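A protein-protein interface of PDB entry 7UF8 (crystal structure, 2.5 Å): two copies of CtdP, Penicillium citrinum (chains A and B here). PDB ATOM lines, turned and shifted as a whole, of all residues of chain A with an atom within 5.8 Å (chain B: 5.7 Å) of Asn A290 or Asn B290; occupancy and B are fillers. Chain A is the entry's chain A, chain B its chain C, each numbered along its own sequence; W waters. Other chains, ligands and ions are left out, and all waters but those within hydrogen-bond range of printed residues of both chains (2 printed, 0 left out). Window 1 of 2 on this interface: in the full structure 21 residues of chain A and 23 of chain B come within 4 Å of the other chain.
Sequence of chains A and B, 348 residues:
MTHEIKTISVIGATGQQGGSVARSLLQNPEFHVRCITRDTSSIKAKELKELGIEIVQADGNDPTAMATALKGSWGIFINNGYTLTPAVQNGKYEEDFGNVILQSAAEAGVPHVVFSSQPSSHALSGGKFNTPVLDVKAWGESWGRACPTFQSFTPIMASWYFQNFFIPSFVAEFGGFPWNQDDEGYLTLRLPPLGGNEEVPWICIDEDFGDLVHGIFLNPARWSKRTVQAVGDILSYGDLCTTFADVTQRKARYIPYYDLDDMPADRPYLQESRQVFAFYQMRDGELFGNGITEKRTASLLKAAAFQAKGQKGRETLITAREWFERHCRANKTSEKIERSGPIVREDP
Of the printed residues of chain B, Gly A289 touches Lys B225 and Arg B226. Asn A290 touches just these residues of chain B: Arg B226 (3.7 Å) and Asn B290 (3.5 Å). Met B157 touches none of the printed residues of chain A. Of the printed residues of chain A, Lys B225 touches Gly A289 (3.9 Å). Of the printed residues of chain A, Glu B286 touches Arg A226. Of the printed residues of chain A, Ile B292 touches Arg A226 (3.5 Å). The nearest residue of chain A that does not touch Asn B290 is Thr A227 (4.1 Å).
Arg A226 touches Glu B286, and with the chains exchanged Glu A286 touches Arg B226. Arg A226 touches Gly B289, and with the chains exchanged Gly A289 touches Arg B226. Arg A226 touches Gly B291, and with the chains exchanged Gly A291 touches Arg B226. Asn B290 touches its own counterpart, Asn A290. 12 positions are printed for both chains.
Printed residues of chain B that touch a printed residue of chain A: Lys B225, Arg B226, Arg B283, Glu B286, Gly B289, Asn B290, Gly B291 and Ile B292. Hydrophobic or aromatic side chains of chain B within 4 Å of the printed part of chain A: Ile B292.
The side-chain amide nitrogen of Gln A229 sits at hydrogen-bond distance from the side-chain amide oxygen of Asn A290 (3.1 Å). The backbone carbonyl oxygen of Ile A292 is in hydrogen-bond range of the side-chain amide nitrogen of Gln A229, 3.0 Å away. The side-chain amide nitrogen (NE2) of Gln B229 lies within hydrogen-bond range of the side-chain amide oxygen (OD1) of Asn B290 (3.3 Å). NE2 of Gln B229 is in hydrogen-bond range of O of Ile B292, at 3.3 Å. O of Gly B289 is in hydrogen-bond range of NH2 of Arg B283 (3.3 Å). The backbone carbonyl oxygen (O) of Phe B288 sits close to the side-chain amide oxygen (OD1) of Asn B290 (3.5 Å).
Among the printed residues, merely in contact across the chains: Lys A225 with Gly B289, Arg A226 with Arg B283, Arg A226 with Gly B289, Arg A226 with Asn B290, Arg A226 with Gly B291, Arg A283 with Arg B226, Gly A289 with Lys B225, Gly A289 with Arg B226, Asn A290 with Arg B226, Asn A290 with Asn B290 and Gly A291 with Arg B226.
NH2 of Arg A226 is in salt-bridge range of OE2 of Glu B286, 2.9 Å away. OE2 of Glu A286 lies within salt-bridge range of NE of Arg B226 (2.7 Å). The guanidinium group (NH2) of Arg A226 sits close to the backbone NH (N) of Ile B292, 3.5 Å away. NH2 of Arg B226 lies close to N of Ile A292.
Water W1 lies within hydrogen-bond range of O of Asn A290 (2.9 Å) and N of Thr B227 (3.2 Å). Water W2 lies within hydrogen-bond range of the backbone NH (N) of Ile A292 (3.2 Å) and the guanidinium group (NH2) of Arg B226 (3.2 Å).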
ATOM      1  N   LEU A 124      14.492  14.808  23.651  1.00  0.00           N
ATOM      2  CA  LEU A 124      13.165  15.399  23.561  1.00  0.00           C
ATOM      3  C   LEU A 124      12.159  14.724  24.478  1.00  0.00           C
ATOM      4  O   LEU A 124      11.158  15.353  24.844  1.00  0.00           O
ATOM      5  CB  LEU A 124      12.655  15.339  22.122  1.00  0.00           C
ATOM      6  CG  LEU A 124      13.131  16.432  21.162  1.00  0.00           C
ATOM      7  CD1 LEU A 124      14.555  16.151  20.696  1.00  0.00           C
ATOM      8  CD2 LEU A 124      12.154  16.556  19.986  1.00  0.00           C
ATOM      9  N   MET A 157      18.306  17.498   7.700  1.00  0.00           N
ATOM     10  CA  MET A 157      17.726  16.244   8.171  1.00  0.00           C
ATOM     11  C   MET A 157      17.032  15.496   7.043  1.00  0.00           C
ATOM     12  O   MET A 157      16.062  15.991   6.476  1.00  0.00           O
ATOM     13  CB  MET A 157      16.726  16.525   9.293  1.00  0.00           C
ATOM     14  CG  MET A 157      17.341  17.089  10.563  1.00  0.00           C
ATOM     15  SD  MET A 157      16.186  16.859  12.116  1.00  0.00           S
ATOM     16  CE  MET A 157      16.920  18.268  13.237  1.00  0.00           C
ATOM     17  N   LYS A 225      22.435  27.742  12.050  1.00  0.00           N
ATOM     18  CA  LYS A 225      21.671  27.366  13.239  1.00  0.00           C
ATOM     19  C   LYS A 225      20.183  27.213  12.950  1.00  0.00           C
ATOM     20  O   LYS A 225      19.361  27.261  13.872  1.00  0.00           O
ATOM     21  CB  LYS A 225      21.866  28.382  14.369  1.00  0.00           C
ATOM     22  CG  LYS A 225      23.294  28.871  14.545  1.00  0.00           C
ATOM     23  CD  LYS A 225      24.187  27.778  15.109  1.00  0.00           C
ATOM     24  CE  LYS A 225      25.614  28.268  15.295  1.00  0.00           C
ATOM     25  NZ  LYS A 225      25.731  29.251  16.405  1.00  0.00           N
ATOM     26  N   ARG A 226      19.820  27.033  11.682  1.00  0.00           N
ATOM     27  CA  ARG A 226      18.432  26.847  11.274  1.00  0.00           C
ATOM     28  C   ARG A 226      18.299  25.471  10.639  1.00  0.00           C
ATOM     29  O   ARG A 226      18.831  25.230   9.550  1.00  0.00           O
ATOM     30  CB  ARG A 226      17.999  27.942  10.301  1.00  0.00           C
ATOM     31  CG  ARG A 226      16.502  28.013  10.063  1.00  0.00           C
ATOM     32  CD  ARG A 226      16.067  27.073   8.953  1.00  0.00           C
ATOM     33  NE  ARG A 226      14.875  27.559   8.264  1.00  0.00           N
ATOM     34  CZ  ARG A 226      14.041  26.792   7.576  1.00  0.00           C
ATOM     35  NH1 ARG A 226      14.233  25.489   7.463  1.00  0.00           N
ATOM     36  NH2 ARG A 226      12.985  27.348   6.988  1.00  0.00           N
ATOM     37  N   THR A 227      17.593  24.575  11.318  1.00  0.00           N
ATOM     38  CA  THR A 227      17.426  23.227  10.801  1.00  0.00           C
ATOM     39  C   THR A 227      16.710  23.256   9.458  1.00  0.00           C
ATOM     40  O   THR A 227      15.701  23.945   9.283  1.00  0.00           O
ATOM     41  CB  THR A 227      16.640  22.366  11.790  1.00  0.00           C
ATOM     42  OG1 THR A 227      17.457  22.077  12.933  1.00  0.00           O
ATOM     43  CG2 THR A 227      16.214  21.067  11.131  1.00  0.00           C
ATOM     44  N   GLN A 229      14.818  20.762   6.716  1.00  0.00           N
ATOM     45  CA  GLN A 229      14.203  19.455   6.518  1.00  0.00           C
ATOM     46  C   GLN A 229      14.291  19.100   5.038  1.00  0.00           C
ATOM     47  O   GLN A 229      13.714  19.797   4.195  1.00  0.00           O
ATOM     48  CB  GLN A 229      12.749  19.464   6.987  1.00  0.00           C
ATOM     49  CG  GLN A 229      12.539  20.010   8.391  1.00  0.00           C
ATOM     50  CD  GLN A 229      11.069  20.113   8.757  1.00  0.00           C
ATOM     51  OE1 GLN A 229      10.195  19.974   7.900  1.00  0.00           O
ATOM     52  NE2 GLN A 229      10.788  20.358  10.034  1.00  0.00           N
ATOM     53  N   ARG A 283       5.452  12.357  19.332  1.00  0.00           N
ATOM     54  CA  ARG A 283       5.515  13.730  18.850  1.00  0.00           C
ATOM     55  C   ARG A 283       4.424  14.055  17.832  1.00  0.00           C
ATOM     56  O   ARG A 283       4.527  15.067  17.127  1.00  0.00           O
ATOM     57  CB  ARG A 283       6.893  14.015  18.249  1.00  0.00           C
ATOM     58  CG  ARG A 283       8.056  13.841  19.220  1.00  0.00           C
ATOM     59  CD  ARG A 283       8.015  14.880  20.324  1.00  0.00           C
ATOM     60  NE  ARG A 283       8.516  16.180  19.895  1.00  0.00           N
ATOM     61  CZ  ARG A 283       9.002  17.103  20.714  1.00  0.00           C
ATOM     62  NH1 ARG A 283       9.076  16.901  22.020  1.00  0.00           N
ATOM     63  NH2 ARG A 283       9.434  18.254  20.210  1.00  0.00           N
ATOM     64  N   GLU A 286       5.735  14.617  14.323  1.00  0.00           N
ATOM     65  CA  GLU A 286       6.756  15.630  14.090  1.00  0.00           C
ATOM     66  C   GLU A 286       8.126  14.970  14.160  1.00  0.00           C
ATOM     67  O   GLU A 286       8.877  15.164  15.120  1.00  0.00           O
ATOM     68  CB  GLU A 286       6.647  16.749  15.118  1.00  0.00           C
ATOM     69  CG  GLU A 286       6.187  18.064  14.533  1.00  0.00           C
ATOM     70  CD  GLU A 286       6.453  19.218  15.468  1.00  0.00           C
ATOM     71  OE1 GLU A 286       7.381  19.105  16.299  1.00  0.00           O
ATOM     72  OE2 GLU A 286       5.734  20.234  15.378  1.00  0.00           O
ATOM     73  N   PHE A 288      10.939  15.371  12.881  1.00  0.00           N
ATOM     74  CA  PHE A 288      12.169  16.152  12.881  1.00  0.00           C
ATOM     75  C   PHE A 288      12.419  16.880  14.194  1.00  0.00           C
ATOM     76  O   PHE A 288      13.567  17.248  14.473  1.00  0.00           O
ATOM     77  CB  PHE A 288      12.153  17.148  11.714  1.00  0.00           C
ATOM     78  CG  PHE A 288      12.218  16.488  10.362  1.00  0.00           C
ATOM     79  CD1 PHE A 288      13.214  15.563  10.081  1.00  0.00           C
ATOM     80  CD2 PHE A 288      11.295  16.790   9.376  1.00  0.00           C
ATOM     81  CE1 PHE A 288      13.281  14.950   8.844  1.00  0.00           C
ATOM     82  CE2 PHE A 288      11.362  16.182   8.135  1.00  0.00           C
ATOM     83  CZ  PHE A 288      12.356  15.261   7.871  1.00  0.00           C
ATOM     84  N   GLY A 289      11.388  17.096  15.009  1.00  0.00           N
ATOM     85  CA  GLY A 289      11.575  17.578  16.357  1.00  0.00           C
ATOM     86  C   GLY A 289      11.734  19.074  16.498  1.00  0.00           C
ATOM     87  O   GLY A 289      11.568  19.598  17.606  1.00  0.00           O
ATOM     88  N   ASN A 290      12.076  19.782  15.420  1.00  0.00           N
ATOM     89  CA  ASN A 290      12.302  21.218  15.489  1.00  0.00           C
ATOM     90  C   ASN A 290      11.047  22.021  15.186  1.00  0.00           C
ATOM     91  O   ASN A 290      10.951  23.180  15.608  1.00  0.00           O
ATOM     92  CB  ASN A 290      13.407  21.631  14.517  1.00  0.00           C
ATOM     93  CG  ASN A 290      12.940  21.648  13.072  1.00  0.00           C
ATOM     94  OD1 ASN A 290      12.575  20.612  12.510  1.00  0.00           O
ATOM     95  ND2 ASN A 290      12.940  22.830  12.465  1.00  0.00           N
ATOM     96  N   GLY A 291      10.090  21.434  14.480  1.00  0.00           N
ATOM     97  CA  GLY A 291       8.916  22.167  14.065  1.00  0.00           C
ATOM     98  C   GLY A 291       8.094  21.333  13.106  1.00  0.00           C
ATOM     99  O   GLY A 291       8.354  20.145  12.908  1.00  0.00           O
ATOM    100  N   ILE A 292       7.089  21.981  12.521  1.00  0.00           N
ATOM    101  CA  ILE A 292       6.202  21.274  11.611  1.00  0.00           C
ATOM    102  C   ILE A 292       7.004  20.749  10.423  1.00  0.00           C
ATOM    103  O   ILE A 292       8.005  21.344  10.003  1.00  0.00           O
ATOM    104  CB  ILE A 292       5.058  22.188  11.140  1.00  0.00           C
ATOM    105  CG1 ILE A 292       5.578  23.248  10.167  1.00  0.00           C
ATOM    106  CG2 ILE A 292       4.398  22.866  12.324  1.00  0.00           C
ATOM    107  CD1 ILE A 292       4.482  24.039   9.483  1.00  0.00           C
ATOM    108  N   MET B 157       8.077  31.834  21.785  1.00  0.00           N
ATOM    109  CA  MET B 157       8.604  33.106  21.305  1.00  0.00           C
ATOM    110  C   MET B 157       7.479  34.049  20.921  1.00  0.00           C
ATOM    111  O   MET B 157       6.725  33.772  19.992  1.00  0.00           O
ATOM    112  CB  MET B 157       9.524  32.880  20.108  1.00  0.00           C
ATOM    113  CG  MET B 157      10.760  32.065  20.431  1.00  0.00           C
ATOM    114  SD  MET B 157      11.988  31.927  18.915  1.00  0.00           S
ATOM    115  CE  MET B 157      13.648  31.638  19.897  1.00  0.00           C
ATOM    116  N   LYS B 225      11.666  20.877  23.849  1.00  0.00           N
ATOM    117  CA  LYS B 225      12.795  21.187  22.974  1.00  0.00           C
ATOM    118  C   LYS B 225      12.361  21.496  21.544  1.00  0.00           C
ATOM    119  O   LYS B 225      13.180  21.461  20.622  1.00  0.00           O
ATOM    120  CB  LYS B 225      13.824  20.048  22.980  1.00  0.00           C
ATOM    121  CG  LYS B 225      13.986  19.336  24.326  1.00  0.00           C
ATOM    122  CD  LYS B 225      14.668  20.229  25.357  1.00  0.00           C
ATOM    123  CE  LYS B 225      15.305  19.434  26.499  1.00  0.00           C
ATOM    124  NZ  LYS B 225      15.973  18.170  26.086  1.00  0.00           N
ATOM    125  N   ARG B 226      11.082  21.805  21.344  1.00  0.00           N
ATOM    126  CA  ARG B 226      10.551  22.195  20.044  1.00  0.00           C
ATOM    127  C   ARG B 226       9.999  23.607  20.189  1.00  0.00           C
ATOM    128  O   ARG B 226       8.978  23.813  20.853  1.00  0.00           O
ATOM    129  CB  ARG B 226       9.472  21.230  19.564  1.00  0.00           C
ATOM    130  CG  ARG B 226       8.852  21.642  18.237  1.00  0.00           C
ATOM    131  CD  ARG B 226       7.388  21.981  18.384  1.00  0.00           C
ATOM    132  NE  ARG B 226       6.714  22.067  17.093  1.00  0.00           N
ATOM    133  CZ  ARG B 226       6.236  23.186  16.565  1.00  0.00           C
ATOM    134  NH1 ARG B 226       6.337  24.347  17.191  1.00  0.00           N
ATOM    135  NH2 ARG B 226       5.635  23.135  15.381  1.00  0.00           N
ATOM    136  N   THR B 227      10.654  24.571  19.549  1.00  0.00           N
ATOM    137  CA  THR B 227      10.242  25.959  19.688  1.00  0.00           C
ATOM    138  C   THR B 227       8.807  26.163  19.214  1.00  0.00           C
ATOM    139  O   THR B 227       8.385  25.626  18.188  1.00  0.00           O
ATOM    140  CB  THR B 227      11.180  26.874  18.896  1.00  0.00           C
ATOM    141  OG1 THR B 227      12.466  26.903  19.524  1.00  0.00           O
ATOM    142  CG2 THR B 227      10.618  28.289  18.837  1.00  0.00           C
ATOM    143  N   VAL B 228       8.065  26.953  19.983  1.00  0.00           N
ATOM    144  CA  VAL B 228       6.694  27.336  19.673  1.00  0.00           C
ATOM    145  C   VAL B 228       6.696  28.830  19.376  1.00  0.00           C
ATOM    146  O   VAL B 228       7.224  29.620  20.167  1.00  0.00           O
ATOM    147  CB  VAL B 228       5.742  27.011  20.836  1.00  0.00           C
ATOM    148  CG1 VAL B 228       4.492  27.882  20.757  1.00  0.00           C
ATOM    149  CG2 VAL B 228       5.380  25.529  20.840  1.00  0.00           C
ATOM    150  N   GLN B 229       6.131  29.212  18.233  1.00  0.00           N
ATOM    151  CA  GLN B 229       6.009  30.610  17.838  1.00  0.00           C
ATOM    152  C   GLN B 229       4.617  31.098  18.226  1.00  0.00           C
ATOM    153  O   GLN B 229       3.615  30.556  17.749  1.00  0.00           O
ATOM    154  CB  GLN B 229       6.251  30.767  16.337  1.00  0.00           C
ATOM    155  CG  GLN B 229       7.540  30.100  15.857  1.00  0.00           C
ATOM    156  CD  GLN B 229       7.672  30.055  14.343  1.00  0.00           C
ATOM    157  OE1 GLN B 229       6.790  30.513  13.613  1.00  0.00           O
ATOM    158  NE2 GLN B 229       8.777  29.490  13.864  1.00  0.00           N
ATOM    159  N   ARG B 283      18.001  37.337   7.596  1.00  0.00           N
ATOM    160  CA  ARG B 283      17.322  36.056   7.703  1.00  0.00           C
ATOM    161  C   ARG B 283      16.120  35.955   6.777  1.00  0.00           C
ATOM    162  O   ARG B 283      15.295  35.052   6.948  1.00  0.00           O
ATOM    163  CB  ARG B 283      16.884  35.817   9.150  1.00  0.00           C
ATOM    164  CG  ARG B 283      18.033  35.642  10.132  1.00  0.00           C
ATOM    165  CD  ARG B 283      18.917  34.456   9.772  1.00  0.00           C
ATOM    166  NE  ARG B 283      18.431  33.218  10.368  1.00  0.00           N
ATOM    167  CZ  ARG B 283      19.205  32.199  10.715  1.00  0.00           C
ATOM    168  NH1 ARG B 283      20.516  32.234  10.538  1.00  0.00           N
ATOM    169  NH2 ARG B 283      18.653  31.120  11.263  1.00  0.00           N
ATOM    170  N   GLU B 286      12.777  35.550   8.434  1.00  0.00           N
ATOM    171  CA  GLU B 286      12.591  34.421   9.347  1.00  0.00           C
ATOM    172  C   GLU B 286      13.095  34.824  10.733  1.00  0.00           C
ATOM    173  O   GLU B 286      14.133  34.374  11.223  1.00  0.00           O
ATOM    174  CB  GLU B 286      13.313  33.190   8.818  1.00  0.00           C
ATOM    175  CG  GLU B 286      12.530  31.906   8.964  1.00  0.00           C
ATOM    176  CD  GLU B 286      13.226  30.737   8.313  1.00  0.00           C
ATOM    177  OE1 GLU B 286      14.357  30.408   8.727  1.00  0.00           O
ATOM    178  OE2 GLU B 286      12.653  30.156   7.368  1.00  0.00           O
ATOM    179  N   PHE B 288      12.307  34.255  13.755  1.00  0.00           N
ATOM    180  CA  PHE B 288      12.381  33.358  14.903  1.00  0.00           C
ATOM    181  C   PHE B 288      13.586  32.427  14.851  1.00  0.00           C
ATOM    182  O   PHE B 288      13.982  31.893  15.894  1.00  0.00           O
ATOM    183  CB  PHE B 288      11.094  32.538  15.018  1.00  0.00           C
ATOM    184  CG  PHE B 288       9.899  33.348  15.438  1.00  0.00           C
ATOM    185  CD1 PHE B 288       9.981  34.233  16.503  1.00  0.00           C
ATOM    186  CD2 PHE B 288       8.693  33.229  14.766  1.00  0.00           C
ATOM    187  CE1 PHE B 288       8.884  34.980  16.892  1.00  0.00           C
ATOM    188  CE2 PHE B 288       7.594  33.974  15.149  1.00  0.00           C
ATOM    189  CZ  PHE B 288       7.690  34.851  16.213  1.00  0.00           C
ATOM    190  N   GLY B 289      14.175  32.225  13.671  1.00  0.00           N
ATOM    191  CA  GLY B 289      15.454  31.564  13.537  1.00  0.00           C
ATOM    192  C   GLY B 289      15.422  30.053  13.465  1.00  0.00           C
ATOM    193  O   GLY B 289      16.401  29.452  13.009  1.00  0.00           O
ATOM    194  N   ASN B 290      14.339  29.417  13.900  1.00  0.00           N
ATOM    195  CA  ASN B 290      14.295  27.961  13.927  1.00  0.00           C
ATOM    196  C   ASN B 290      13.722  27.355  12.656  1.00  0.00           C
ATOM    197  O   ASN B 290      14.009  26.188  12.357  1.00  0.00           O
ATOM    198  CB  ASN B 290      13.457  27.481  15.113  1.00  0.00           C
ATOM    199  CG  ASN B 290      12.057  28.071  15.112  1.00  0.00           C
ATOM    200  OD1 ASN B 290      11.876  29.282  14.973  1.00  0.00           O
ATOM    201  ND2 ASN B 290      11.053  27.208  15.238  1.00  0.00           N
ATOM    202  N   GLY B 291      12.928  28.110  11.909  1.00  0.00           N
ATOM    203  CA  GLY B 291      12.243  27.577  10.752  1.00  0.00           C
ATOM    204  C   GLY B 291      11.265  28.605  10.224  1.00  0.00           C
ATOM    205  O   GLY B 291      11.231  29.746  10.689  1.00  0.00           O
ATOM    206  N   ILE B 292      10.450  28.176   9.254  1.00  0.00           N
ATOM    207  CA  ILE B 292       9.534  29.120   8.627  1.00  0.00           C
ATOM    208  C   ILE B 292       8.581  29.672   9.683  1.00  0.00           C
ATOM    209  O   ILE B 292       8.232  28.993  10.658  1.00  0.00           O
ATOM    210  CB  ILE B 292       8.745  28.482   7.471  1.00  0.00           C
ATOM    211  CG1 ILE B 292       8.198  27.111   7.871  1.00  0.00           C
ATOM    212  CG2 ILE B 292       9.612  28.381   6.223  1.00  0.00           C
ATOM    213  CD1 ILE B 292       7.034  26.650   7.007  1.00  0.00           C
HETATM  214  O   HOH W   1      12.979  23.535  17.666  1.00  0.00           O
HETATM  215  O   HOH W   2       6.933  25.082  13.193  1.00  0.00           O
